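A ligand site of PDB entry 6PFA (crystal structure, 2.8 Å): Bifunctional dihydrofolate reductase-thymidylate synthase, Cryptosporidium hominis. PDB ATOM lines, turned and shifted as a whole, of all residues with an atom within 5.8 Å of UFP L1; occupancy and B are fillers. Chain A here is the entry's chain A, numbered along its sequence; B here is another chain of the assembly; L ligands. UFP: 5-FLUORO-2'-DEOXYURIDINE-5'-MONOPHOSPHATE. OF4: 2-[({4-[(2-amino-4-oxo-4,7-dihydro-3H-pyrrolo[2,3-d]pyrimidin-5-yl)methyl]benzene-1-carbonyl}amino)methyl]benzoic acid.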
ATOM      1  N   ASN A 256       1.317 -16.534 -21.254  1.00  0.00           N
ATOM      2  CA  ASN A 256       0.767 -17.692 -21.960  1.00  0.00           C
ATOM      3  C   ASN A 256      -0.170 -17.196 -23.061  1.00  0.00           C
ATOM      4  O   ASN A 256      -0.243 -16.003 -23.351  1.00  0.00           O
ATOM      5  CB  ASN A 256       0.088 -18.651 -20.970  1.00  0.00           C
ATOM      6  CG  ASN A 256      -1.007 -17.990 -20.148  1.00  0.00           C
ATOM      7  OD1 ASN A 256      -1.786 -17.180 -20.650  1.00  0.00           O
ATOM      8  ND2 ASN A 256      -1.055 -18.319 -18.862  1.00  0.00           N
ATOM      9  N   ARG A 257      -0.882 -18.143 -23.672  1.00  0.00           N
ATOM     10  CA  ARG A 257      -1.750 -17.829 -24.815  1.00  0.00           C
ATOM     11  C   ARG A 257      -2.889 -16.897 -24.448  1.00  0.00           C
ATOM     12  O   ARG A 257      -3.498 -16.298 -25.349  1.00  0.00           O
ATOM     13  CB  ARG A 257      -2.310 -19.124 -25.397  1.00  0.00           C
ATOM     14  CG  ARG A 257      -3.105 -19.941 -24.400  1.00  0.00           C
ATOM     15  CD  ARG A 257      -3.830 -21.104 -25.048  1.00  0.00           C
ATOM     16  NE  ARG A 257      -4.709 -21.771 -24.095  1.00  0.00           N
ATOM     17  CZ  ARG A 257      -5.945 -21.366 -23.812  1.00  0.00           C
ATOM     18  NH1 ARG A 257      -6.455 -20.303 -24.419  1.00  0.00           N
ATOM     19  NH2 ARG A 257      -6.678 -22.031 -22.931  1.00  0.00           N
ATOM     20  N   GLU A 294     -20.177 -32.856 -16.184  1.00  0.00           N
ATOM     21  CA  GLU A 294     -19.093 -32.888 -17.170  1.00  0.00           C
ATOM     22  C   GLU A 294     -18.500 -34.282 -17.288  1.00  0.00           C
ATOM     23  O   GLU A 294     -18.124 -34.707 -18.393  1.00  0.00           O
ATOM     24  CB  GLU A 294     -18.000 -31.879 -16.789  1.00  0.00           C
ATOM     25  CG  GLU A 294     -16.832 -31.850 -17.760  1.00  0.00           C
ATOM     26  CD  GLU A 294     -15.590 -31.205 -17.166  1.00  0.00           C
ATOM     27  OE1 GLU A 294     -15.452 -31.204 -15.929  1.00  0.00           O
ATOM     28  OE2 GLU A 294     -14.748 -30.695 -17.940  1.00  0.00           O
ATOM     29  N   TRP A 316     -17.675 -24.838 -20.204  1.00  0.00           N
ATOM     30  CA  TRP A 316     -17.116 -24.912 -21.548  1.00  0.00           C
ATOM     31  C   TRP A 316     -17.681 -23.831 -22.474  1.00  0.00           C
ATOM     32  O   TRP A 316     -17.581 -23.969 -23.701  1.00  0.00           O
ATOM     33  CB  TRP A 316     -17.357 -26.294 -22.150  1.00  0.00           C
ATOM     34  CG  TRP A 316     -16.451 -27.353 -21.591  1.00  0.00           C
ATOM     35  CD1 TRP A 316     -16.741 -28.245 -20.606  1.00  0.00           C
ATOM     36  CD2 TRP A 316     -15.089 -27.594 -21.984  1.00  0.00           C
ATOM     37  NE1 TRP A 316     -15.652 -29.050 -20.365  1.00  0.00           N
ATOM     38  CE2 TRP A 316     -14.624 -28.670 -21.190  1.00  0.00           C
ATOM     39  CE3 TRP A 316     -14.231 -27.023 -22.912  1.00  0.00           C
ATOM     40  CZ2 TRP A 316     -13.337 -29.183 -21.317  1.00  0.00           C
ATOM     41  CZ3 TRP A 316     -12.943 -27.536 -23.040  1.00  0.00           C
ATOM     42  CH2 TRP A 316     -12.513 -28.598 -22.248  1.00  0.00           C
ATOM     43  N   TYR A 342     -11.951 -34.847 -24.874  1.00  0.00           N
ATOM     44  CA  TYR A 342     -12.346 -35.825 -23.873  1.00  0.00           C
ATOM     45  C   TYR A 342     -13.697 -36.425 -24.235  1.00  0.00           C
ATOM     46  O   TYR A 342     -14.628 -35.723 -24.643  1.00  0.00           O
ATOM     47  CB  TYR A 342     -12.426 -35.211 -22.475  1.00  0.00           C
ATOM     48  CG  TYR A 342     -11.382 -34.171 -22.122  1.00  0.00           C
ATOM     49  CD1 TYR A 342     -10.093 -34.539 -21.756  1.00  0.00           C
ATOM     50  CD2 TYR A 342     -11.713 -32.828 -22.071  1.00  0.00           C
ATOM     51  CE1 TYR A 342      -9.154 -33.584 -21.386  1.00  0.00           C
ATOM     52  CE2 TYR A 342     -10.788 -31.860 -21.712  1.00  0.00           C
ATOM     53  CZ  TYR A 342      -9.510 -32.252 -21.373  1.00  0.00           C
ATOM     54  OH  TYR A 342      -8.579 -31.296 -21.010  1.00  0.00           O
ATOM     55  N   LEU A 399      -9.489 -27.107 -27.663  1.00  0.00           N
ATOM     56  CA  LEU A 399      -8.452 -26.969 -26.651  1.00  0.00           C
ATOM     57  C   LEU A 399      -7.853 -28.340 -26.381  1.00  0.00           C
ATOM     58  O   LEU A 399      -8.594 -29.298 -26.124  1.00  0.00           O
ATOM     59  CB  LEU A 399      -9.022 -26.347 -25.372  1.00  0.00           C
ATOM     60  CG  LEU A 399      -8.021 -25.910 -24.303  1.00  0.00           C
ATOM     61  CD1 LEU A 399      -7.065 -24.861 -24.855  1.00  0.00           C
ATOM     62  CD2 LEU A 399      -8.738 -25.387 -23.074  1.00  0.00           C
ATOM     63  N   PRO A 400      -6.527 -28.486 -26.469  1.00  0.00           N
ATOM     64  CA  PRO A 400      -5.912 -29.798 -26.246  1.00  0.00           C
ATOM     65  C   PRO A 400      -6.202 -30.312 -24.849  1.00  0.00           C
ATOM     66  O   PRO A 400      -6.485 -29.531 -23.927  1.00  0.00           O
ATOM     67  CB  PRO A 400      -4.418 -29.527 -26.444  1.00  0.00           C
ATOM     68  CG  PRO A 400      -4.392 -28.351 -27.349  1.00  0.00           C
ATOM     69  CD  PRO A 400      -5.548 -27.500 -26.927  1.00  0.00           C
ATOM     70  N   CYS A 402      -6.054 -31.378 -21.101  1.00  0.00           N
ATOM     71  CA  CYS A 402      -5.232 -31.033 -19.949  1.00  0.00           C
ATOM     72  C   CYS A 402      -4.958 -32.252 -19.074  1.00  0.00           C
ATOM     73  O   CYS A 402      -3.786 -32.568 -18.807  1.00  0.00           O
ATOM     74  CB  CYS A 402      -5.923 -29.937 -19.129  1.00  0.00           C
ATOM     75  SG  CYS A 402      -6.158 -28.433 -20.069  1.00  0.00           S
ATOM     76  N   HIS A 403      -6.002 -32.950 -18.640  1.00  0.00           N
ATOM     77  CA  HIS A 403      -5.800 -34.284 -18.075  1.00  0.00           C
ATOM     78  C   HIS A 403      -5.575 -35.221 -19.258  1.00  0.00           C
ATOM     79  O   HIS A 403      -6.518 -35.583 -19.967  1.00  0.00           O
ATOM     80  CB  HIS A 403      -6.969 -34.716 -17.182  1.00  0.00           C
ATOM     81  CG  HIS A 403      -8.321 -34.315 -17.682  1.00  0.00           C
ATOM     82  ND1 HIS A 403      -9.248 -35.234 -18.132  1.00  0.00           N
ATOM     83  CD2 HIS A 403      -8.933 -33.109 -17.740  1.00  0.00           C
ATOM     84  CE1 HIS A 403     -10.352 -34.610 -18.475  1.00  0.00           C
ATOM     85  NE2 HIS A 403     -10.185 -33.319 -18.250  1.00  0.00           N
ATOM     86  N   GLN A 422      -1.373 -34.613 -15.658  1.00  0.00           N
ATOM     87  CA  GLN A 422      -2.008 -33.378 -16.099  1.00  0.00           C
ATOM     88  C   GLN A 422      -0.925 -32.444 -16.645  1.00  0.00           C
ATOM     89  O   GLN A 422      -0.045 -32.014 -15.890  1.00  0.00           O
ATOM     90  CB  GLN A 422      -2.761 -32.724 -14.942  1.00  0.00           C
ATOM     91  CG  GLN A 422      -3.708 -31.605 -15.327  1.00  0.00           C
ATOM     92  CD  GLN A 422      -4.568 -31.149 -14.155  1.00  0.00           C
ATOM     93  OE1 GLN A 422      -4.608 -31.798 -13.117  1.00  0.00           O
ATOM     94  NE2 GLN A 422      -5.259 -30.024 -14.335  1.00  0.00           N
ATOM     95  N   ARG A 423      -1.000 -32.133 -17.936  1.00  0.00           N
ATOM     96  CA  ARG A 423       0.035 -31.304 -18.552  1.00  0.00           C
ATOM     97  C   ARG A 423      -0.048 -29.851 -18.100  1.00  0.00           C
ATOM     98  O   ARG A 423       0.994 -29.182 -17.983  1.00  0.00           O
ATOM     99  CB  ARG A 423      -0.059 -31.392 -20.084  1.00  0.00           C
ATOM    100  CG  ARG A 423      -1.363 -30.857 -20.660  1.00  0.00           C
ATOM    101  CD  ARG A 423      -1.198 -30.432 -22.113  1.00  0.00           C
ATOM    102  NE  ARG A 423      -2.413 -29.813 -22.639  1.00  0.00           N
ATOM    103  CZ  ARG A 423      -2.676 -28.508 -22.586  1.00  0.00           C
ATOM    104  NH1 ARG A 423      -1.806 -27.676 -22.036  1.00  0.00           N
ATOM    105  NH2 ARG A 423      -3.802 -28.034 -23.089  1.00  0.00           N
ATOM    106  N   SER A 424      -1.250 -29.352 -17.842  1.00  0.00           N
ATOM    107  CA  SER A 424      -1.454 -27.962 -17.427  1.00  0.00           C
ATOM    108  C   SER A 424      -2.556 -27.938 -16.391  1.00  0.00           C
ATOM    109  O   SER A 424      -3.592 -28.575 -16.566  1.00  0.00           O
ATOM    110  CB  SER A 424      -1.825 -27.080 -18.620  1.00  0.00           C
ATOM    111  OG  SER A 424      -1.897 -25.719 -18.224  1.00  0.00           O
ATOM    112  N   CYS A 425      -2.340 -27.186 -15.304  1.00  0.00           N
ATOM    113  CA  CYS A 425      -3.228 -27.247 -14.152  1.00  0.00           C
ATOM    114  C   CYS A 425      -3.518 -25.834 -13.662  1.00  0.00           C
ATOM    115  O   CYS A 425      -2.659 -25.201 -13.038  1.00  0.00           O
ATOM    116  CB  CYS A 425      -2.603 -28.096 -13.037  1.00  0.00           C
ATOM    117  SG  CYS A 425      -3.610 -28.223 -11.553  1.00  0.00           S
ATOM    118  N   ASP A 426      -4.734 -25.361 -13.923  1.00  0.00           N
ATOM    119  CA  ASP A 426      -5.244 -24.136 -13.317  1.00  0.00           C
ATOM    120  C   ASP A 426      -5.579 -24.451 -11.869  1.00  0.00           C
ATOM    121  O   ASP A 426      -6.634 -25.010 -11.565  1.00  0.00           O
ATOM    122  CB  ASP A 426      -6.463 -23.632 -14.077  1.00  0.00           C
ATOM    123  CG  ASP A 426      -7.034 -22.343 -13.505  1.00  0.00           C
ATOM    124  OD1 ASP A 426      -6.486 -21.818 -12.511  1.00  0.00           O
ATOM    125  OD2 ASP A 426      -8.049 -21.860 -14.056  1.00  0.00           O
ATOM    126  N   LEU A 427      -4.685 -24.077 -10.946  1.00  0.00           N
ATOM    127  CA  LEU A 427      -4.843 -24.450  -9.548  1.00  0.00           C
ATOM    128  C   LEU A 427      -6.024 -23.759  -8.882  1.00  0.00           C
ATOM    129  O   LEU A 427      -6.474 -24.219  -7.828  1.00  0.00           O
ATOM    130  CB  LEU A 427      -3.559 -24.141  -8.780  1.00  0.00           C
ATOM    131  CG  LEU A 427      -2.372 -25.075  -9.063  1.00  0.00           C
ATOM    132  CD1 LEU A 427      -1.123 -24.581  -8.385  1.00  0.00           C
ATOM    133  CD2 LEU A 427      -2.710 -26.490  -8.603  1.00  0.00           C
ATOM    134  N   GLY A 430      -9.455 -25.309 -12.384  1.00  0.00           N
ATOM    135  CA  GLY A 430      -9.449 -26.653 -12.933  1.00  0.00           C
ATOM    136  C   GLY A 430      -9.053 -27.707 -11.914  1.00  0.00           C
ATOM    137  O   GLY A 430      -9.608 -28.807 -11.899  1.00  0.00           O
ATOM    138  N   SER A 431      -8.069 -27.397 -11.066  1.00  0.00           N
ATOM    139  CA  SER A 431      -7.541 -28.404 -10.138  1.00  0.00           C
ATOM    140  C   SER A 431      -8.599 -28.934  -9.169  1.00  0.00           C
ATOM    141  O   SER A 431      -8.724 -30.157  -9.049  1.00  0.00           O
ATOM    142  CB  SER A 431      -6.330 -27.829  -9.391  1.00  0.00           C
ATOM    143  OG  SER A 431      -5.608 -28.856  -8.751  1.00  0.00           O
ATOM    144  N   ASN A 434     -10.595 -31.199 -11.279  1.00  0.00           N
ATOM    145  CA  ASN A 434      -9.894 -32.421 -11.684  1.00  0.00           C
ATOM    146  C   ASN A 434      -9.797 -33.412 -10.536  1.00  0.00           C
ATOM    147  O   ASN A 434      -9.906 -34.621 -10.740  1.00  0.00           O
ATOM    148  CB  ASN A 434      -8.501 -32.074 -12.209  1.00  0.00           C
ATOM    149  CG  ASN A 434      -8.545 -31.414 -13.566  1.00  0.00           C
ATOM    150  OD1 ASN A 434      -8.069 -30.287 -13.730  1.00  0.00           O
ATOM    151  ND2 ASN A 434      -9.105 -32.104 -14.550  1.00  0.00           N
ATOM    152  N   HIS A 464       0.221 -23.905 -12.208  1.00  0.00           N
ATOM    153  CA  HIS A 464       0.303 -22.454 -12.271  1.00  0.00           C
ATOM    154  C   HIS A 464      -0.894 -21.807 -11.585  1.00  0.00           C
ATOM    155  O   HIS A 464      -1.908 -22.456 -11.309  1.00  0.00           O
ATOM    156  CB  HIS A 464       0.415 -21.984 -13.726  1.00  0.00           C
ATOM    157  CG  HIS A 464      -0.628 -22.553 -14.632  1.00  0.00           C
ATOM    158  ND1 HIS A 464      -1.915 -22.061 -14.697  1.00  0.00           N
ATOM    159  CD2 HIS A 464      -0.590 -23.599 -15.496  1.00  0.00           C
ATOM    160  CE1 HIS A 464      -2.618 -22.761 -15.568  1.00  0.00           C
ATOM    161  NE2 HIS A 464      -1.843 -23.696 -16.062  1.00  0.00           N
ATOM    162  N   TYR A 466      -3.117 -18.178 -12.041  1.00  0.00           N
ATOM    163  CA  TYR A 466      -3.369 -16.954 -12.801  1.00  0.00           C
ATOM    164  C   TYR A 466      -3.305 -15.744 -11.879  1.00  0.00           C
ATOM    165  O   TYR A 466      -3.732 -15.806 -10.728  1.00  0.00           O
ATOM    166  CB  TYR A 466      -4.715 -17.025 -13.501  1.00  0.00           C
ATOM    167  CG  TYR A 466      -4.719 -17.971 -14.689  1.00  0.00           C
ATOM    168  CD1 TYR A 466      -4.957 -19.324 -14.526  1.00  0.00           C
ATOM    169  CD2 TYR A 466      -4.446 -17.499 -15.971  1.00  0.00           C
ATOM    170  CE1 TYR A 466      -4.948 -20.190 -15.611  1.00  0.00           C
ATOM    171  CE2 TYR A 466      -4.436 -18.355 -17.054  1.00  0.00           C
ATOM    172  CZ  TYR A 466      -4.687 -19.700 -16.874  1.00  0.00           C
ATOM    173  OH  TYR A 466      -4.669 -20.549 -17.948  1.00  0.00           O
ATOM    174  N   ASP B 381       4.958 -22.327 -24.299  1.00  0.00           N
ATOM    175  CA  ASP B 381       3.819 -23.173 -24.607  1.00  0.00           C
ATOM    176  C   ASP B 381       3.748 -24.339 -23.632  1.00  0.00           C
ATOM    177  O   ASP B 381       4.770 -24.887 -23.218  1.00  0.00           O
ATOM    178  CB  ASP B 381       3.919 -23.679 -26.041  1.00  0.00           C
ATOM    179  CG  ASP B 381       2.743 -24.542 -26.452  1.00  0.00           C
ATOM    180  OD1 ASP B 381       1.592 -24.063 -26.367  1.00  0.00           O
ATOM    181  OD2 ASP B 381       2.973 -25.685 -26.882  1.00  0.00           O
ATOM    182  N   ARG B 382       2.529 -24.717 -23.238  1.00  0.00           N
ATOM    183  CA  ARG B 382       2.311 -25.767 -22.260  1.00  0.00           C
ATOM    184  C   ARG B 382       1.894 -27.083 -22.905  1.00  0.00           C
ATOM    185  O   ARG B 382       1.182 -27.880 -22.291  1.00  0.00           O
ATOM    186  CB  ARG B 382       1.277 -25.317 -21.233  1.00  0.00           C
ATOM    187  CG  ARG B 382       1.717 -24.079 -20.469  1.00  0.00           C
ATOM    188  CD  ARG B 382       0.663 -23.566 -19.492  1.00  0.00           C
ATOM    189  NE  ARG B 382      -0.458 -22.961 -20.193  1.00  0.00           N
ATOM    190  CZ  ARG B 382      -1.237 -22.011 -19.674  1.00  0.00           C
ATOM    191  NH1 ARG B 382      -0.999 -21.544 -18.453  1.00  0.00           N
ATOM    192  NH2 ARG B 382      -2.247 -21.516 -20.382  1.00  0.00           N
ATOM    193  N   ARG B 383       2.348 -27.335 -24.137  1.00  0.00           N
ATOM    194  CA  ARG B 383       1.927 -28.515 -24.890  1.00  0.00           C
ATOM    195  C   ARG B 383       3.106 -29.267 -25.510  1.00  0.00           C
ATOM    196  O   ARG B 383       2.921 -29.993 -26.484  1.00  0.00           O
ATOM    197  CB  ARG B 383       0.925 -28.138 -25.984  1.00  0.00           C
ATOM    198  CG  ARG B 383      -0.234 -27.290 -25.497  1.00  0.00           C
ATOM    199  CD  ARG B 383      -1.122 -26.870 -26.645  1.00  0.00           C
ATOM    200  NE  ARG B 383      -2.348 -26.228 -26.176  1.00  0.00           N
ATOM    201  CZ  ARG B 383      -2.601 -24.933 -26.277  1.00  0.00           C
ATOM    202  NH1 ARG B 383      -1.699 -24.123 -26.839  1.00  0.00           N
ATOM    203  NH2 ARG B 383      -3.740 -24.438 -25.828  1.00  0.00           N
HETATM  204  N1  UFP L   1      -7.346 -26.609 -17.215  1.00  0.00           N
HETATM  205  C2  UFP L   1      -7.200 -27.392 -16.105  1.00  0.00           C
HETATM  206  N3  UFP L   1      -7.927 -28.522 -15.965  1.00  0.00           N
HETATM  207  C4  UFP L   1      -8.822 -28.903 -16.904  1.00  0.00           C
HETATM  208  C5  UFP L   1      -8.998 -28.100 -18.051  1.00  0.00           C
HETATM  209  C6  UFP L   1      -8.263 -26.975 -18.171  1.00  0.00           C
HETATM  210  O2  UFP L   1      -6.416 -27.137 -15.201  1.00  0.00           O
HETATM  211  O4  UFP L   1      -9.469 -29.918 -16.759  1.00  0.00           O
HETATM  212  F5  UFP L   1      -9.878 -28.447 -19.013  1.00  0.00           F
HETATM  213  C1' UFP L   1      -6.627 -25.352 -17.523  1.00  0.00           C
HETATM  214  C2' UFP L   1      -5.093 -25.403 -17.371  1.00  0.00           C
HETATM  215  C3' UFP L   1      -4.694 -24.163 -18.202  1.00  0.00           C
HETATM  216  C4' UFP L   1      -5.699 -24.210 -19.377  1.00  0.00           C
HETATM  217  O3' UFP L   1      -4.905 -22.965 -17.450  1.00  0.00           O
HETATM  218  O4' UFP L   1      -6.791 -25.069 -18.938  1.00  0.00           O
HETATM  219  C5' UFP L   1      -5.029 -24.740 -20.649  1.00  0.00           C
HETATM  220  O5' UFP L   1      -4.203 -23.720 -21.200  1.00  0.00           O
HETATM  221  P   UFP L   1      -3.118 -24.379 -22.180  1.00  0.00           P
HETATM  222  O1P UFP L   1      -2.369 -23.312 -22.876  1.00  0.00           O
HETATM  223  O2P UFP L   1      -3.868 -25.294 -23.281  1.00  0.00           O
HETATM  224  O3P UFP L   1      -2.089 -25.281 -21.341  1.00  0.00           O
HETATM  225  C10 OF4 L   2     -13.866 -24.859 -13.945  1.00  0.00           C
HETATM  226  C11 OF4 L   2     -14.438 -23.693 -14.527  1.00  0.00           C
HETATM  227  C21 OF4 L   2     -15.298 -22.213  -9.736  1.00  0.00           C
HETATM  228  C22 OF4 L   2     -19.068 -22.996 -10.118  1.00  0.00           C
HETATM  229  C1  OF4 L   2     -10.195 -24.259 -19.151  1.00  0.00           C
HETATM  230  C12 OF4 L   2     -14.278 -23.486 -15.917  1.00  0.00           C
HETATM  231  C13 OF4 L   2     -13.579 -24.414 -16.709  1.00  0.00           C
HETATM  232  C14 OF4 L   2     -15.193 -22.668 -13.734  1.00  0.00           C
HETATM  233  C15 OF4 L   2     -16.655 -22.150 -11.840  1.00  0.00           C
HETATM  234  C16 OF4 L   2     -16.568 -22.393 -10.340  1.00  0.00           C
HETATM  235  C17 OF4 L   2     -17.684 -22.790  -9.543  1.00  0.00           C
HETATM  236  C18 OF4 L   2     -17.487 -22.979  -8.153  1.00  0.00           C
HETATM  237  C19 OF4 L   2     -16.218 -22.797  -7.563  1.00  0.00           C
HETATM  238  C2  OF4 L   2     -10.568 -24.705 -17.902  1.00  0.00           C
HETATM  239  C20 OF4 L   2     -15.124 -22.419  -8.355  1.00  0.00           C
HETATM  240  C3  OF4 L   2      -9.928 -24.058 -16.743  1.00  0.00           C
HETATM  241  C4  OF4 L   2      -8.727 -22.724 -18.353  1.00  0.00           C
HETATM  242  C5  OF4 L   2     -11.537 -25.745 -18.093  1.00  0.00           C
HETATM  243  C6  OF4 L   2     -11.716 -25.891 -19.452  1.00  0.00           C
HETATM  244  C7  OF4 L   2     -12.254 -26.532 -17.021  1.00  0.00           C
HETATM  245  C8  OF4 L   2     -13.014 -25.568 -16.131  1.00  0.00           C
HETATM  246  C9  OF4 L   2     -13.160 -25.786 -14.745  1.00  0.00           C
HETATM  247  N1  OF4 L   2      -9.267 -23.268 -19.409  1.00  0.00           N
HETATM  248  N2  OF4 L   2      -9.032 -23.088 -17.033  1.00  0.00           N
HETATM  249  N3  OF4 L   2     -10.890 -24.978 -20.084  1.00  0.00           N
HETATM  250  N4  OF4 L   2      -7.797 -21.716 -18.392  1.00  0.00           N
HETATM  251  N5  OF4 L   2     -15.879 -23.080 -12.658  1.00  0.00           N
HETATM  252  O1  OF4 L   2     -10.182 -24.376 -15.574  1.00  0.00           O
HETATM  253  O2  OF4 L   2     -15.173 -21.490 -14.089  1.00  0.00           O
HETATM  254  O3  OF4 L   2     -19.158 -24.027 -11.001  1.00  0.00           O
HETATM  255  O4  OF4 L   2     -20.037 -22.304  -9.803  1.00  0.00           O
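NH1 of Arg 382 of chain B lies within hydrogen-bond range of NE2 of His 464 (3.3 Å).
The guanidinium group (NH1) of Arg 382 of chain B lies close to the side-chain amide nitrogen (ND2) of Asn 256 (3.3 Å).
OD1 of Asn 434 sits at hydrogen-bond distance from NE2 of Gln 422 (2.9 Å).
NH1 of Arg 423 is in hydrogen-bond range of O of Arg 382 of chain B (3.0 Å).
The side-chain sulfur of Cys 425 lies close to the side-chain hydroxyl of Ser 431.
The backbone NH (N) of Cys 402 lies within hydrogen-bond range of the side-chain hydroxyl (OH) of Tyr 342, at 2.5 Å.
The backbone NH (N) of His 464 sits at hydrogen-bond distance from the backbone carbonyl oxygen (O) of Cys 425, at 3.3 Å.
The backbone carbonyl oxygen (O) of Gly 430 lies close to the side-chain amide oxygen (OD1) of Asn 434 (2.8 Å).
OH of Tyr 466 lies within hydrogen-bond range of N4 of OF4 L2 (3.4 Å).
O3' of UFP L1 sits at hydrogen-bond distance from OH of Tyr 466.
An oxygen (O3') of UFP L1 lies close to a ring nitrogen (NE2) of His 464 (3.4 Å).
An oxygen (O1P) of UFP L1 lies within salt-bridge range of the guanidinium group of Arg 257 (3.1 Å).
The guanidinium group (NE) of Arg 382 of chain B lies within salt-bridge range of an oxygen (O3P) of UFP L1, at 3.1 Å.
The side-chain amide oxygen of Asn 434 is in hydrogen-bond range of a nitrogen (N3) of UFP L1, at 2.9 Å.
O2P of UFP L1 lies within salt-bridge range of NH2 of Arg 383 of chain B, at 2.7 Å.
OG of Ser 424 sits at hydrogen-bond distance from O3P of UFP L1 (3.2 Å).
The guanidinium group of Arg 423 lies within salt-bridge range of an oxygen (O3P) of UFP L1 (2.5 Å).
O2 of UFP L1 lies within hydrogen-bond range of N of Asp 426, 2.8 Å away.
The side-chain sulfur of Cys 402 sits close to an oxygen (O4') of UFP L1, at 3.6 Å.
An oxygen (O2) of UFP L1 sits at hydrogen-bond distance from the side-chain amide nitrogen (NE2) of Gln 422.
A nitrogen (N2) of OF4 L2 sits at hydrogen-bond distance from the side-chain carboxylate of Asp 426 (3.4 Å).
An oxygen (O1) of OF4 L2 is in hydrogen-bond range of the backbone NH (N) of Gly 430, at 3.4 Å.
Residues that only touch UFP L1: Tyr 342 (3.7 Å), Leu 399 (3.6 Å), His 403 (3.4 Å), Cys 425 (3.4 Å) and Gly 430 (3.8 Å).
Within 4 Å of UFP L1: Arg 257, Tyr 342, Leu 399, Cys 402, His 403, Gln 422, Arg 423, Ser 424, Cys 425, Asp 426, Gly 430, Asn 434, His 464, Tyr 466, Arg 382 of chain B and Arg 383 of chain B.
A nitrogen (N4) of OF4 L2 lies within hydrogen-bond range of an oxygen (O3') of UFP L1 (3.3 Å).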
